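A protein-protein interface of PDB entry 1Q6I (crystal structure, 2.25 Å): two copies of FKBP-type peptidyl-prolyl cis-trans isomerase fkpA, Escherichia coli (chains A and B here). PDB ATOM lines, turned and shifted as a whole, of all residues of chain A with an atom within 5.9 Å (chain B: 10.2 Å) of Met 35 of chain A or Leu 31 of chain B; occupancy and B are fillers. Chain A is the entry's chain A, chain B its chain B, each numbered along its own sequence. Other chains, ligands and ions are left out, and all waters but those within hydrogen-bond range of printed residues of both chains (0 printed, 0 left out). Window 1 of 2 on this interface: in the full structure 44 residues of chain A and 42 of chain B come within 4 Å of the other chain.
Of the 13 printed residues of chain A, 8 touch a printed residue of chain B. Hydrophobic or aromatic side chains of chain A within 4 Å of the printed part of chain B: Leu 31, Met 35, Leu 39, Leu 54 and Val 58. Of the 26 printed residues of chain B, 9 touch a printed residue of chain A. Hydrophobic or aromatic side chains of chain B that line the printed part of chain A: Leu 31, Met 35, Ala 61 and Phe 62. Among the printed residues, 12 pairs touch across the chains. Among the printed residues, no Asp or Glu carboxylate lies within 4 Å of a Lys or Arg side-chain nitrogen of the other chain.
Leu 31 of chain A touches Met 35 of chain B, and with the chains exchanged Met 35 of chain A touches Leu 31 of chain B. Val 58 of chain A touches Gly 32 of chain B, but with the chains exchanged Gly 32 of chain A does not touch Val 58 of chain B (4.2 Å). Positions printed for both chains: 30, 31, 32, 33, 34, 35, 36, 37, 38, 39, 54 and 58. Of the 12 pairs that touch across the chains among the printed residues, 2 have their exchanged pair printed and touching as well.
Printed residues of chain B within 4 Å of Met 35 of chain A: Leu 31 (3.5 Å). Printed residues of chain A within 4 Å of Leu 31 of chain B: Met 35 (3.5 Å). Printed residues of chain A within 4 Å of Ala 61 of chain B: Gly 32, Arg 33 and Glu 36. Printed residues of chain A within 4 Å of Gly 32 of chain B: Val 58. Of the printed residues of chain B, Val 58 of chain A touches Gly 28, Ala 29 and Gly 32. Of the printed residues of chain A, Asp 64 of chain B touches Glu 36 (2.4 Å). Of the printed residues of chain B, Leu 54 of chain A touches Ala 24 and Gly 28. Leu 39 of chain B touches none of the printed residues of chain A. The nearest printed residue of chain A that does not touch Met 35 of chain B is Val 58 of chain A (4.2 Å).
OD1 of Asp 64 of chain B lies close to OE1 of Glu 36 of chain A (2.4 Å). The backbone NH (N) of Val 58 of chain A sits close to the backbone carbonyl oxygen (O) of Gly 28 of chain B (3.4 Å). OE1 of Glu 36 of chain A lies close to O of Ala 61 of chain B (3.4 Å).
NE of Arg 33 of chain A lies within hydrogen-bond range of OD1 of Asn 37 of chain A, at 3.2 Å. The side-chain hydroxyl (OG) of Ser 38 of chain A lies within hydrogen-bond range of the backbone carbonyl oxygen (O) of Met 35 of chain A, 3.3 Å away. The side-chain carboxylate of Glu 36 of chain A is in salt-bridge range of the side-chain amino group of Lys 40 of chain A (3.9 Å).
CG of Met 35 of chain B touches CD1 of Leu 31 of chain A, 3.7 Å away. Gly 32 of chain A touches Ala 61 of chain B (C to CB, 3.9 Å). Ala 61 of chain B touches Arg 33 of chain A. CG of Met 35 of chain A touches CD2 of Leu 31 of chain B, 3.5 Å away. CD2 of Leu 39 of chain A touches CZ of Phe 62 of chain B, at 3.4 Å. CA of Leu 54 of chain A touches O of Ala 24 of chain B (3.6 Å). CA of Gly 28 of chain B touches O of Leu 54 of chain A (3.4 Å). Ala 29 of chain B touches Val 58 of chain A. Gly 32 of chain B touches Val 58 of chain A (CA to O, 3.9 Å).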
ATOM      1  N   SER A  30     -14.018  10.139 -10.594  1.00  0.00           N
ATOM      2  CA  SER A  30     -13.591   8.841 -11.065  1.00  0.00           C
ATOM      3  C   SER A  30     -12.088   8.613 -10.806  1.00  0.00           C
ATOM      4  O   SER A  30     -11.668   7.507 -10.477  1.00  0.00           O
ATOM      5  CB  SER A  30     -13.898   8.711 -12.548  1.00  0.00           C
ATOM      6  OG  SER A  30     -13.530   7.433 -13.018  1.00  0.00           O
ATOM      7  N   LEU A  31     -11.282   9.650 -10.948  1.00  0.00           N
ATOM      8  CA  LEU A  31      -9.869   9.513 -10.692  1.00  0.00           C
ATOM      9  C   LEU A  31      -9.591   9.410  -9.223  1.00  0.00           C
ATOM     10  O   LEU A  31      -8.764   8.642  -8.789  1.00  0.00           O
ATOM     11  CB  LEU A  31      -9.105  10.704 -11.223  1.00  0.00           C
ATOM     12  CG  LEU A  31      -8.901  10.712 -12.719  1.00  0.00           C
ATOM     13  CD1 LEU A  31      -8.429  12.092 -13.199  1.00  0.00           C
ATOM     14  CD2 LEU A  31      -7.930   9.621 -13.101  1.00  0.00           C
ATOM     15  N   GLY A  32     -10.240  10.232  -8.449  1.00  0.00           N
ATOM     16  CA  GLY A  32     -10.015  10.221  -7.023  1.00  0.00           C
ATOM     17  C   GLY A  32     -10.509   8.947  -6.379  1.00  0.00           C
ATOM     18  O   GLY A  32      -9.997   8.508  -5.354  1.00  0.00           O
ATOM     19  N   ARG A  33     -11.519   8.350  -6.972  1.00  0.00           N
ATOM     20  CA  ARG A  33     -12.037   7.095  -6.459  1.00  0.00           C
ATOM     21  C   ARG A  33     -11.017   5.990  -6.757  1.00  0.00           C
ATOM     22  O   ARG A  33     -10.791   5.087  -5.958  1.00  0.00           O
ATOM     23  CB  ARG A  33     -13.389   6.837  -7.103  1.00  0.00           C
ATOM     24  CG  ARG A  33     -13.726   5.414  -7.355  1.00  0.00           C
ATOM     25  CD  ARG A  33     -14.522   4.762  -6.268  1.00  0.00           C
ATOM     26  NE  ARG A  33     -14.814   3.406  -6.714  1.00  0.00           N
ATOM     27  CZ  ARG A  33     -15.648   2.573  -6.138  1.00  0.00           C
ATOM     28  NH1 ARG A  33     -16.316   2.931  -5.050  1.00  0.00           N
ATOM     29  NH2 ARG A  33     -15.809   1.369  -6.666  1.00  0.00           N
ATOM     30  N   TYR A  34     -10.394   6.092  -7.919  1.00  0.00           N
ATOM     31  CA  TYR A  34      -9.335   5.176  -8.315  1.00  0.00           C
ATOM     32  C   TYR A  34      -8.165   5.210  -7.329  1.00  0.00           C
ATOM     33  O   TYR A  34      -7.617   4.170  -6.972  1.00  0.00           O
ATOM     34  CB  TYR A  34      -8.808   5.567  -9.687  1.00  0.00           C
ATOM     35  CG  TYR A  34      -7.466   4.945 -10.014  1.00  0.00           C
ATOM     36  CD1 TYR A  34      -7.376   3.636 -10.470  1.00  0.00           C
ATOM     37  CD2 TYR A  34      -6.290   5.666  -9.867  1.00  0.00           C
ATOM     38  CE1 TYR A  34      -6.153   3.062 -10.767  1.00  0.00           C
ATOM     39  CE2 TYR A  34      -5.052   5.095 -10.158  1.00  0.00           C
ATOM     40  CZ  TYR A  34      -5.000   3.800 -10.610  1.00  0.00           C
ATOM     41  OH  TYR A  34      -3.780   3.245 -10.907  1.00  0.00           O
ATOM     42  N   MET A  35      -7.786   6.414  -6.915  1.00  0.00           N
ATOM     43  CA  MET A  35      -6.709   6.600  -5.962  1.00  0.00           C
ATOM     44  C   MET A  35      -7.054   5.970  -4.628  1.00  0.00           C
ATOM     45  O   MET A  35      -6.235   5.287  -4.021  1.00  0.00           O
ATOM     46  CB  MET A  35      -6.449   8.088  -5.698  1.00  0.00           C
ATOM     47  CG  MET A  35      -5.819   8.881  -6.832  1.00  0.00           C
ATOM     48  SD  MET A  35      -3.885   8.712  -6.979  1.00  0.00           S
ATOM     49  CE  MET A  35      -3.869   7.630  -8.507  1.00  0.00           C
ATOM     50  N   GLU A  36      -8.256   6.253  -4.156  1.00  0.00           N
ATOM     51  CA  GLU A  36      -8.700   5.765  -2.864  1.00  0.00           C
ATOM     52  C   GLU A  36      -8.713   4.253  -2.849  1.00  0.00           C
ATOM     53  O   GLU A  36      -8.373   3.645  -1.847  1.00  0.00           O
ATOM     54  CB  GLU A  36     -10.083   6.285  -2.511  1.00  0.00           C
ATOM     55  CG  GLU A  36     -10.182   6.733  -1.073  1.00  0.00           C
ATOM     56  CD  GLU A  36     -11.554   6.478  -0.517  1.00  0.00           C
ATOM     57  OE1 GLU A  36     -12.529   6.664  -1.287  1.00  0.00           O
ATOM     58  OE2 GLU A  36     -11.671   6.075   0.666  1.00  0.00           O
ATOM     59  N   ASN A  37      -9.113   3.651  -3.958  1.00  0.00           N
ATOM     60  CA  ASN A  37      -9.105   2.211  -4.048  1.00  0.00           C
ATOM     61  C   ASN A  37      -7.683   1.633  -3.950  1.00  0.00           C
ATOM     62  O   ASN A  37      -7.470   0.619  -3.304  1.00  0.00           O
ATOM     63  CB  ASN A  37      -9.840   1.762  -5.311  1.00  0.00           C
ATOM     64  CG  ASN A  37     -11.369   1.906  -5.186  1.00  0.00           C
ATOM     65  OD1 ASN A  37     -12.101   1.795  -6.173  1.00  0.00           O
ATOM     66  ND2 ASN A  37     -11.841   2.170  -3.971  1.00  0.00           N
ATOM     67  N   SER A  38      -6.697   2.278  -4.550  1.00  0.00           N
ATOM     68  CA  SER A  38      -5.305   1.803  -4.420  1.00  0.00           C
ATOM     69  C   SER A  38      -4.731   1.974  -2.996  1.00  0.00           C
ATOM     70  O   SER A  38      -3.943   1.155  -2.522  1.00  0.00           O
ATOM     71  CB  SER A  38      -4.404   2.558  -5.394  1.00  0.00           C
ATOM     72  OG  SER A  38      -5.171   3.270  -6.347  1.00  0.00           O
ATOM     73  N   LEU A  39      -5.095   3.069  -2.350  1.00  0.00           N
ATOM     74  CA  LEU A  39      -4.691   3.327  -0.982  1.00  0.00           C
ATOM     75  C   LEU A  39      -5.351   2.313  -0.041  1.00  0.00           C
ATOM     76  O   LEU A  39      -4.753   1.879   0.919  1.00  0.00           O
ATOM     77  CB  LEU A  39      -5.073   4.751  -0.558  1.00  0.00           C
ATOM     78  CG  LEU A  39      -3.994   5.837  -0.546  1.00  0.00           C
ATOM     79  CD1 LEU A  39      -3.408   6.079  -1.895  1.00  0.00           C
ATOM     80  CD2 LEU A  39      -4.565   7.145  -0.045  1.00  0.00           C
ATOM     81  N   LYS A  40      -6.578   1.921  -0.330  1.00  0.00           N
ATOM     82  CA  LYS A  40      -7.225   0.914   0.492  1.00  0.00           C
ATOM     83  C   LYS A  40      -6.467  -0.414   0.438  1.00  0.00           C
ATOM     84  O   LYS A  40      -6.409  -1.142   1.428  1.00  0.00           O
ATOM     85  CB  LYS A  40      -8.699   0.730   0.099  1.00  0.00           C
ATOM     86  CG  LYS A  40      -9.628   1.840   0.608  1.00  0.00           C
ATOM     87  CD  LYS A  40     -11.110   1.603   0.210  1.00  0.00           C
ATOM     88  CE  LYS A  40     -11.733   2.905  -0.310  1.00  0.00           C
ATOM     89  NZ  LYS A  40     -12.734   2.743  -1.422  1.00  0.00           N
ATOM     90  N   LEU A  54      -1.281  13.934  -0.004  1.00  0.00           N
ATOM     91  CA  LEU A  54      -1.674  13.451  -1.313  1.00  0.00           C
ATOM     92  C   LEU A  54      -2.455  14.512  -2.052  1.00  0.00           C
ATOM     93  O   LEU A  54      -2.166  14.792  -3.206  1.00  0.00           O
ATOM     94  CB  LEU A  54      -2.470  12.165  -1.237  1.00  0.00           C
ATOM     95  CG  LEU A  54      -2.508  11.574  -2.622  1.00  0.00           C
ATOM     96  CD1 LEU A  54      -2.400  10.098  -2.597  1.00  0.00           C
ATOM     97  CD2 LEU A  54      -3.732  12.012  -3.371  1.00  0.00           C
ATOM     98  N   VAL A  58      -1.627  16.789  -5.541  1.00  0.00           N
ATOM     99  CA  VAL A  58      -2.557  16.922  -6.629  1.00  0.00           C
ATOM    100  C   VAL A  58      -2.680  18.377  -6.998  1.00  0.00           C
ATOM    101  O   VAL A  58      -2.474  18.728  -8.127  1.00  0.00           O
ATOM    102  CB  VAL A  58      -3.953  16.368  -6.274  1.00  0.00           C
ATOM    103  CG1 VAL A  58      -4.948  16.733  -7.377  1.00  0.00           C
ATOM    104  CG2 VAL A  58      -3.899  14.875  -6.093  1.00  0.00           C
ATOM    105  N   SER B  23       5.979  10.088  -0.327  1.00  0.00           N
ATOM    106  CA  SER B  23       5.355   9.236  -1.318  1.00  0.00           C
ATOM    107  C   SER B  23       3.934   9.645  -1.567  1.00  0.00           C
ATOM    108  O   SER B  23       3.446   9.562  -2.685  1.00  0.00           O
ATOM    109  CB  SER B  23       5.392   7.769  -0.894  1.00  0.00           C
ATOM    110  OG  SER B  23       6.720   7.312  -0.899  1.00  0.00           O
ATOM    111  N   ALA B  24       3.242  10.057  -0.519  1.00  0.00           N
ATOM    112  CA  ALA B  24       1.871  10.489  -0.721  1.00  0.00           C
ATOM    113  C   ALA B  24       1.867  11.692  -1.676  1.00  0.00           C
ATOM    114  O   ALA B  24       1.169  11.675  -2.680  1.00  0.00           O
ATOM    115  CB  ALA B  24       1.196  10.831   0.612  1.00  0.00           C
ATOM    116  N   TYR B  25       2.654  12.725  -1.370  1.00  0.00           N
ATOM    117  CA  TYR B  25       2.725  13.923  -2.220  1.00  0.00           C
ATOM    118  C   TYR B  25       3.092  13.556  -3.664  1.00  0.00           C
ATOM    119  O   TYR B  25       2.445  14.012  -4.611  1.00  0.00           O
ATOM    120  CB  TYR B  25       3.738  14.913  -1.657  1.00  0.00           C
ATOM    121  CG  TYR B  25       3.751  16.270  -2.310  1.00  0.00           C
ATOM    122  CD1 TYR B  25       4.534  16.517  -3.430  1.00  0.00           C
ATOM    123  CD2 TYR B  25       3.012  17.324  -1.785  1.00  0.00           C
ATOM    124  CE1 TYR B  25       4.574  17.785  -4.014  1.00  0.00           C
ATOM    125  CE2 TYR B  25       3.055  18.590  -2.360  1.00  0.00           C
ATOM    126  CZ  TYR B  25       3.846  18.801  -3.471  1.00  0.00           C
ATOM    127  OH  TYR B  25       3.880  20.016  -4.051  1.00  0.00           O
ATOM    128  N   ALA B  26       4.093  12.695  -3.822  1.00  0.00           N
ATOM    129  CA  ALA B  26       4.482  12.242  -5.145  1.00  0.00           C
ATOM    130  C   ALA B  26       3.350  11.553  -5.890  1.00  0.00           C
ATOM    131  O   ALA B  26       3.125  11.825  -7.081  1.00  0.00           O
ATOM    132  CB  ALA B  26       5.648  11.311  -5.063  1.00  0.00           C
ATOM    133  N   LEU B  27       2.657  10.643  -5.197  1.00  0.00           N
ATOM    134  CA  LEU B  27       1.562   9.955  -5.820  1.00  0.00           C
ATOM    135  C   LEU B  27       0.523  10.994  -6.237  1.00  0.00           C
ATOM    136  O   LEU B  27       0.010  10.933  -7.331  1.00  0.00           O
ATOM    137  CB  LEU B  27       0.953   8.915  -4.898  1.00  0.00           C
ATOM    138  CG  LEU B  27       1.024   7.434  -5.249  1.00  0.00           C
ATOM    139  CD1 LEU B  27       0.385   6.617  -4.153  1.00  0.00           C
ATOM    140  CD2 LEU B  27       0.350   7.134  -6.540  1.00  0.00           C
ATOM    141  N   GLY B  28       0.231  11.965  -5.375  1.00  0.00           N
ATOM    142  CA  GLY B  28      -0.695  13.034  -5.737  1.00  0.00           C
ATOM    143  C   GLY B  28      -0.237  13.957  -6.884  1.00  0.00           C
ATOM    144  O   GLY B  28      -1.020  14.320  -7.774  1.00  0.00           O
ATOM    145  N   ALA B  29       1.018  14.399  -6.801  1.00  0.00           N
ATOM    146  CA  ALA B  29       1.644  15.198  -7.841  1.00  0.00           C
ATOM    147  C   ALA B  29       1.527  14.484  -9.173  1.00  0.00           C
ATOM    148  O   ALA B  29       1.242  15.066 -10.195  1.00  0.00           O
ATOM    149  CB  ALA B  29       3.120  15.411  -7.509  1.00  0.00           C
ATOM    150  N   SER B  30       1.695  13.180  -9.137  1.00  0.00           N
ATOM    151  CA  SER B  30       1.638  12.378 -10.329  1.00  0.00           C
ATOM    152  C   SER B  30       0.227  12.313 -10.959  1.00  0.00           C
ATOM    153  O   SER B  30       0.065  12.231 -12.187  1.00  0.00           O
ATOM    154  CB  SER B  30       2.143  11.004  -9.964  1.00  0.00           C
ATOM    155  OG  SER B  30       1.951  10.154 -11.043  1.00  0.00           O
ATOM    156  N   LEU B  31      -0.795  12.330 -10.117  1.00  0.00           N
ATOM    157  CA  LEU B  31      -2.160  12.362 -10.620  1.00  0.00           C
ATOM    158  C   LEU B  31      -2.419  13.782 -11.160  1.00  0.00           C
ATOM    159  O   LEU B  31      -3.027  13.953 -12.193  1.00  0.00           O
ATOM    160  CB  LEU B  31      -3.145  11.971  -9.510  1.00  0.00           C
ATOM    161  CG  LEU B  31      -4.623  12.247  -9.787  1.00  0.00           C
ATOM    162  CD1 LEU B  31      -5.055  11.480 -10.988  1.00  0.00           C
ATOM    163  CD2 LEU B  31      -5.498  11.863  -8.604  1.00  0.00           C
ATOM    164  N   GLY B  32      -1.937  14.798 -10.465  1.00  0.00           N
ATOM    165  CA  GLY B  32      -2.023  16.156 -10.981  1.00  0.00           C
ATOM    166  C   GLY B  32      -1.441  16.256 -12.393  1.00  0.00           C
ATOM    167  O   GLY B  32      -2.124  16.580 -13.369  1.00  0.00           O
ATOM    168  N   ARG B  33      -0.151  15.994 -12.482  1.00  0.00           N
ATOM    169  CA  ARG B  33       0.526  15.867 -13.739  1.00  0.00           C
ATOM    170  C   ARG B  33      -0.386  15.263 -14.773  1.00  0.00           C
ATOM    171  O   ARG B  33      -0.626  15.831 -15.845  1.00  0.00           O
ATOM    172  CB  ARG B  33       1.658  14.879 -13.569  1.00  0.00           C
ATOM    173  CG  ARG B  33       2.067  14.264 -14.860  1.00  0.00           C
ATOM    174  CD  ARG B  33       2.657  15.295 -15.751  1.00  0.00           C
ATOM    175  NE  ARG B  33       3.789  15.846 -15.031  1.00  0.00           N
ATOM    176  CZ  ARG B  33       4.233  17.075 -15.132  1.00  0.00           C
ATOM    177  NH1 ARG B  33       3.648  17.952 -15.940  1.00  0.00           N
ATOM    178  NH2 ARG B  33       5.287  17.413 -14.418  1.00  0.00           N
ATOM    179  N   TYR B  34      -0.861  14.070 -14.451  1.00  0.00           N
ATOM    180  CA  TYR B  34      -1.660  13.296 -15.378  1.00  0.00           C
ATOM    181  C   TYR B  34      -2.931  14.042 -15.806  1.00  0.00           C
ATOM    182  O   TYR B  34      -3.378  13.934 -16.949  1.00  0.00           O
ATOM    183  CB  TYR B  34      -2.049  11.955 -14.755  1.00  0.00           C
ATOM    184  CG  TYR B  34      -3.056  11.197 -15.583  1.00  0.00           C
ATOM    185  CD1 TYR B  34      -2.657  10.332 -16.615  1.00  0.00           C
ATOM    186  CD2 TYR B  34      -4.418  11.367 -15.357  1.00  0.00           C
ATOM    187  CE1 TYR B  34      -3.587   9.662 -17.362  1.00  0.00           C
ATOM    188  CE2 TYR B  34      -5.331  10.721 -16.088  1.00  0.00           C
ATOM    189  CZ  TYR B  34      -4.932   9.869 -17.092  1.00  0.00           C
ATOM    190  OH  TYR B  34      -5.913   9.213 -17.786  1.00  0.00           O
ATOM    191  N   MET B  35      -3.531  14.775 -14.886  1.00  0.00           N
ATOM    192  CA  MET B  35      -4.744  15.491 -15.256  1.00  0.00           C
ATOM    193  C   MET B  35      -4.418  16.654 -16.151  1.00  0.00           C
ATOM    194  O   MET B  35      -5.154  16.922 -17.097  1.00  0.00           O
ATOM    195  CB  MET B  35      -5.451  16.047 -14.009  1.00  0.00           C
ATOM    196  CG  MET B  35      -6.181  15.026 -13.123  1.00  0.00           C
ATOM    197  SD  MET B  35      -6.211  15.535 -11.236  1.00  0.00           S
ATOM    198  CE  MET B  35      -7.301  17.044 -11.330  1.00  0.00           C
ATOM    199  N   GLU B  36      -3.335  17.355 -15.841  1.00  0.00           N
ATOM    200  CA  GLU B  36      -2.879  18.432 -16.716  1.00  0.00           C
ATOM    201  C   GLU B  36      -2.573  17.907 -18.134  1.00  0.00           C
ATOM    202  O   GLU B  36      -3.046  18.485 -19.107  1.00  0.00           O
ATOM    203  CB  GLU B  36      -1.681  19.179 -16.131  1.00  0.00           C
ATOM    204  CG  GLU B  36      -2.043  20.278 -15.132  1.00  0.00           C
ATOM    205  CD  GLU B  36      -2.847  21.433 -15.746  1.00  0.00           C
ATOM    206  OE1 GLU B  36      -3.267  22.365 -15.009  1.00  0.00           O
ATOM    207  OE2 GLU B  36      -3.076  21.422 -16.975  1.00  0.00           O
ATOM    208  N   ASN B  37      -1.818  16.811 -18.262  1.00  0.00           N
ATOM    209  CA  ASN B  37      -1.538  16.245 -19.593  1.00  0.00           C
ATOM    210  C   ASN B  37      -2.803  15.901 -20.355  1.00  0.00           C
ATOM    211  O   ASN B  37      -2.946  16.169 -21.556  1.00  0.00           O
ATOM    212  CB  ASN B  37      -0.697  14.982 -19.504  1.00  0.00           C
ATOM    213  CG  ASN B  37       0.750  15.264 -19.153  1.00  0.00           C
ATOM    214  OD1 ASN B  37       1.301  16.307 -19.502  1.00  0.00           O
ATOM    215  ND2 ASN B  37       1.380  14.320 -18.472  1.00  0.00           N
ATOM    216  N   SER B  38      -3.735  15.306 -19.645  1.00  0.00           N
ATOM    217  CA  SER B  38      -5.004  14.936 -20.250  1.00  0.00           C
ATOM    218  C   SER B  38      -5.796  16.156 -20.790  1.00  0.00           C
ATOM    219  O   SER B  38      -6.275  16.134 -21.915  1.00  0.00           O
ATOM    220  CB  SER B  38      -5.834  14.183 -19.228  1.00  0.00           C
ATOM    221  OG  SER B  38      -7.077  13.928 -19.807  1.00  0.00           O
ATOM    222  N   LEU B  39      -5.957  17.184 -19.960  1.00  0.00           N
ATOM    223  CA  LEU B  39      -6.574  18.446 -20.364  1.00  0.00           C
ATOM    224  C   LEU B  39      -5.909  19.022 -21.609  1.00  0.00           C
ATOM    225  O   LEU B  39      -6.567  19.634 -22.459  1.00  0.00           O
ATOM    226  CB  LEU B  39      -6.394  19.476 -19.281  1.00  0.00           C
ATOM    227  CG  LEU B  39      -7.113  19.234 -17.993  1.00  0.00           C
ATOM    228  CD1 LEU B  39      -6.672  20.307 -17.082  1.00  0.00           C
ATOM    229  CD2 LEU B  39      -8.638  19.265 -18.226  1.00  0.00           C
ATOM    230  N   LEU B  54     -12.990  19.809 -11.758  1.00  0.00           N
ATOM    231  CA  LEU B  54     -12.199  18.592 -11.812  1.00  0.00           C
ATOM    232  C   LEU B  54     -11.526  18.292 -10.438  1.00  0.00           C
ATOM    233  O   LEU B  54     -11.546  17.153  -9.927  1.00  0.00           O
ATOM    234  CB  LEU B  54     -11.173  18.722 -12.918  1.00  0.00           C
ATOM    235  CG  LEU B  54     -10.203  17.587 -13.180  1.00  0.00           C
ATOM    236  CD1 LEU B  54     -10.835  16.337 -13.688  1.00  0.00           C
ATOM    237  CD2 LEU B  54      -9.175  18.083 -14.217  1.00  0.00           C
ATOM    238  N   ILE B  55     -10.964  19.318  -9.820  1.00  0.00           N
ATOM    239  CA  ILE B  55     -10.308  19.144  -8.533  1.00  0.00           C
ATOM    240  C   ILE B  55     -11.337  18.780  -7.474  1.00  0.00           C
ATOM    241  O   ILE B  55     -11.103  17.874  -6.687  1.00  0.00           O
ATOM    242  CB  ILE B  55      -9.511  20.424  -8.136  1.00  0.00           C
ATOM    243  CG1 ILE B  55      -8.048  20.265  -8.540  1.00  0.00           C
ATOM    244  CG2 ILE B  55      -9.467  20.644  -6.628  1.00  0.00           C
ATOM    245  CD1 ILE B  55      -7.840  20.196  -9.992  1.00  0.00           C
ATOM    246  N   GLY B  57     -14.041  17.207  -7.632  1.00  0.00           N
ATOM    247  CA  GLY B  57     -14.441  15.823  -7.746  1.00  0.00           C
ATOM    248  C   GLY B  57     -13.418  14.905  -7.092  1.00  0.00           C
ATOM    249  O   GLY B  57     -13.763  13.894  -6.455  1.00  0.00           O
ATOM    250  N   VAL B  58     -12.157  15.267  -7.274  1.00  0.00           N
ATOM    251  CA  VAL B  58     -11.051  14.495  -6.745  1.00  0.00           C
ATOM    252  C   VAL B  58     -11.067  14.548  -5.237  1.00  0.00           C
ATOM    253  O   VAL B  58     -10.952  13.510  -4.571  1.00  0.00           O
ATOM    254  CB  VAL B  58      -9.685  15.027  -7.215  1.00  0.00           C
ATOM    255  CG1 VAL B  58      -8.531  14.405  -6.336  1.00  0.00           C
ATOM    256  CG2 VAL B  58      -9.498  14.741  -8.695  1.00  0.00           C
ATOM    257  N   GLN B  59     -11.211  15.755  -4.697  1.00  0.00           N
ATOM    258  CA  GLN B  59     -11.255  15.928  -3.242  1.00  0.00           C
ATOM    259  C   GLN B  59     -12.472  15.205  -2.652  1.00  0.00           C
ATOM    260  O   GLN B  59     -12.337  14.403  -1.707  1.00  0.00           O
ATOM    261  CB  GLN B  59     -11.301  17.408  -2.893  1.00  0.00           C
ATOM    262  CG  GLN B  59     -10.024  18.122  -3.279  1.00  0.00           C
ATOM    263  CD  GLN B  59     -10.140  19.619  -3.258  1.00  0.00           C
ATOM    264  OE1 GLN B  59     -11.231  20.174  -3.433  1.00  0.00           O
ATOM    265  NE2 GLN B  59      -9.006  20.289  -3.095  1.00  0.00           N
ATOM    266  N   ALA B  61     -14.227  12.764  -3.816  1.00  0.00           N
ATOM    267  CA  ALA B  61     -14.099  11.311  -3.848  1.00  0.00           C
ATOM    268  C   ALA B  61     -13.102  10.841  -2.846  1.00  0.00           C
ATOM    269  O   ALA B  61     -13.333   9.895  -2.134  1.00  0.00           O
ATOM    270  CB  ALA B  61     -13.694  10.842  -5.212  1.00  0.00           C
ATOM    271  N   PHE B  62     -11.973  11.516  -2.785  1.00  0.00           N
ATOM    272  CA  PHE B  62     -10.917  11.090  -1.887  1.00  0.00           C
ATOM    273  C   PHE B  62     -11.363  11.123  -0.440  1.00  0.00           C
ATOM    274  O   PHE B  62     -10.737  10.490   0.408  1.00  0.00           O
ATOM    275  CB  PHE B  62      -9.682  11.974  -2.075  1.00  0.00           C
ATOM    276  CG  PHE B  62      -8.423  11.354  -1.580  1.00  0.00           C
ATOM    277  CD1 PHE B  62      -8.022  10.112  -2.035  1.00  0.00           C
ATOM    278  CD2 PHE B  62      -7.649  11.999  -0.642  1.00  0.00           C
ATOM    279  CE1 PHE B  62      -6.854   9.525  -1.571  1.00  0.00           C
ATOM    280  CE2 PHE B  62      -6.480  11.423  -0.176  1.00  0.00           C
ATOM    281  CZ  PHE B  62      -6.080  10.180  -0.646  1.00  0.00           C
ATOM    282  N   ALA B  63     -12.430  11.867  -0.164  1.00  0.00           N
ATOM    283  CA  ALA B  63     -12.989  11.954   1.177  1.00  0.00           C
ATOM    284  C   ALA B  63     -14.356  11.280   1.237  1.00  0.00           C
ATOM    285  O   ALA B  63     -15.082  11.431   2.209  1.00  0.00           O
ATOM    286  CB  ALA B  63     -13.113  13.392   1.597  1.00  0.00           C
ATOM    287  N   ASP B  64     -14.715  10.567   0.176  1.00  0.00           N
ATOM    288  CA  ASP B  64     -15.989   9.853   0.118  1.00  0.00           C
ATOM    289  C   ASP B  64     -17.255  10.721   0.193  1.00  0.00           C
ATOM    290  O   ASP B  64     -18.227  10.343   0.829  1.00  0.00           O
ATOM    291  CB  ASP B  64     -15.984   8.772   1.197  1.00  0.00           C
ATOM    292  CG  ASP B  64     -14.630   8.074   1.295  1.00  0.00           C
ATOM    293  OD1 ASP B  64     -14.153   7.591   0.237  1.00  0.00           O
ATOM    294  OD2 ASP B  64     -13.945   8.007   2.353  1.00  0.00           O
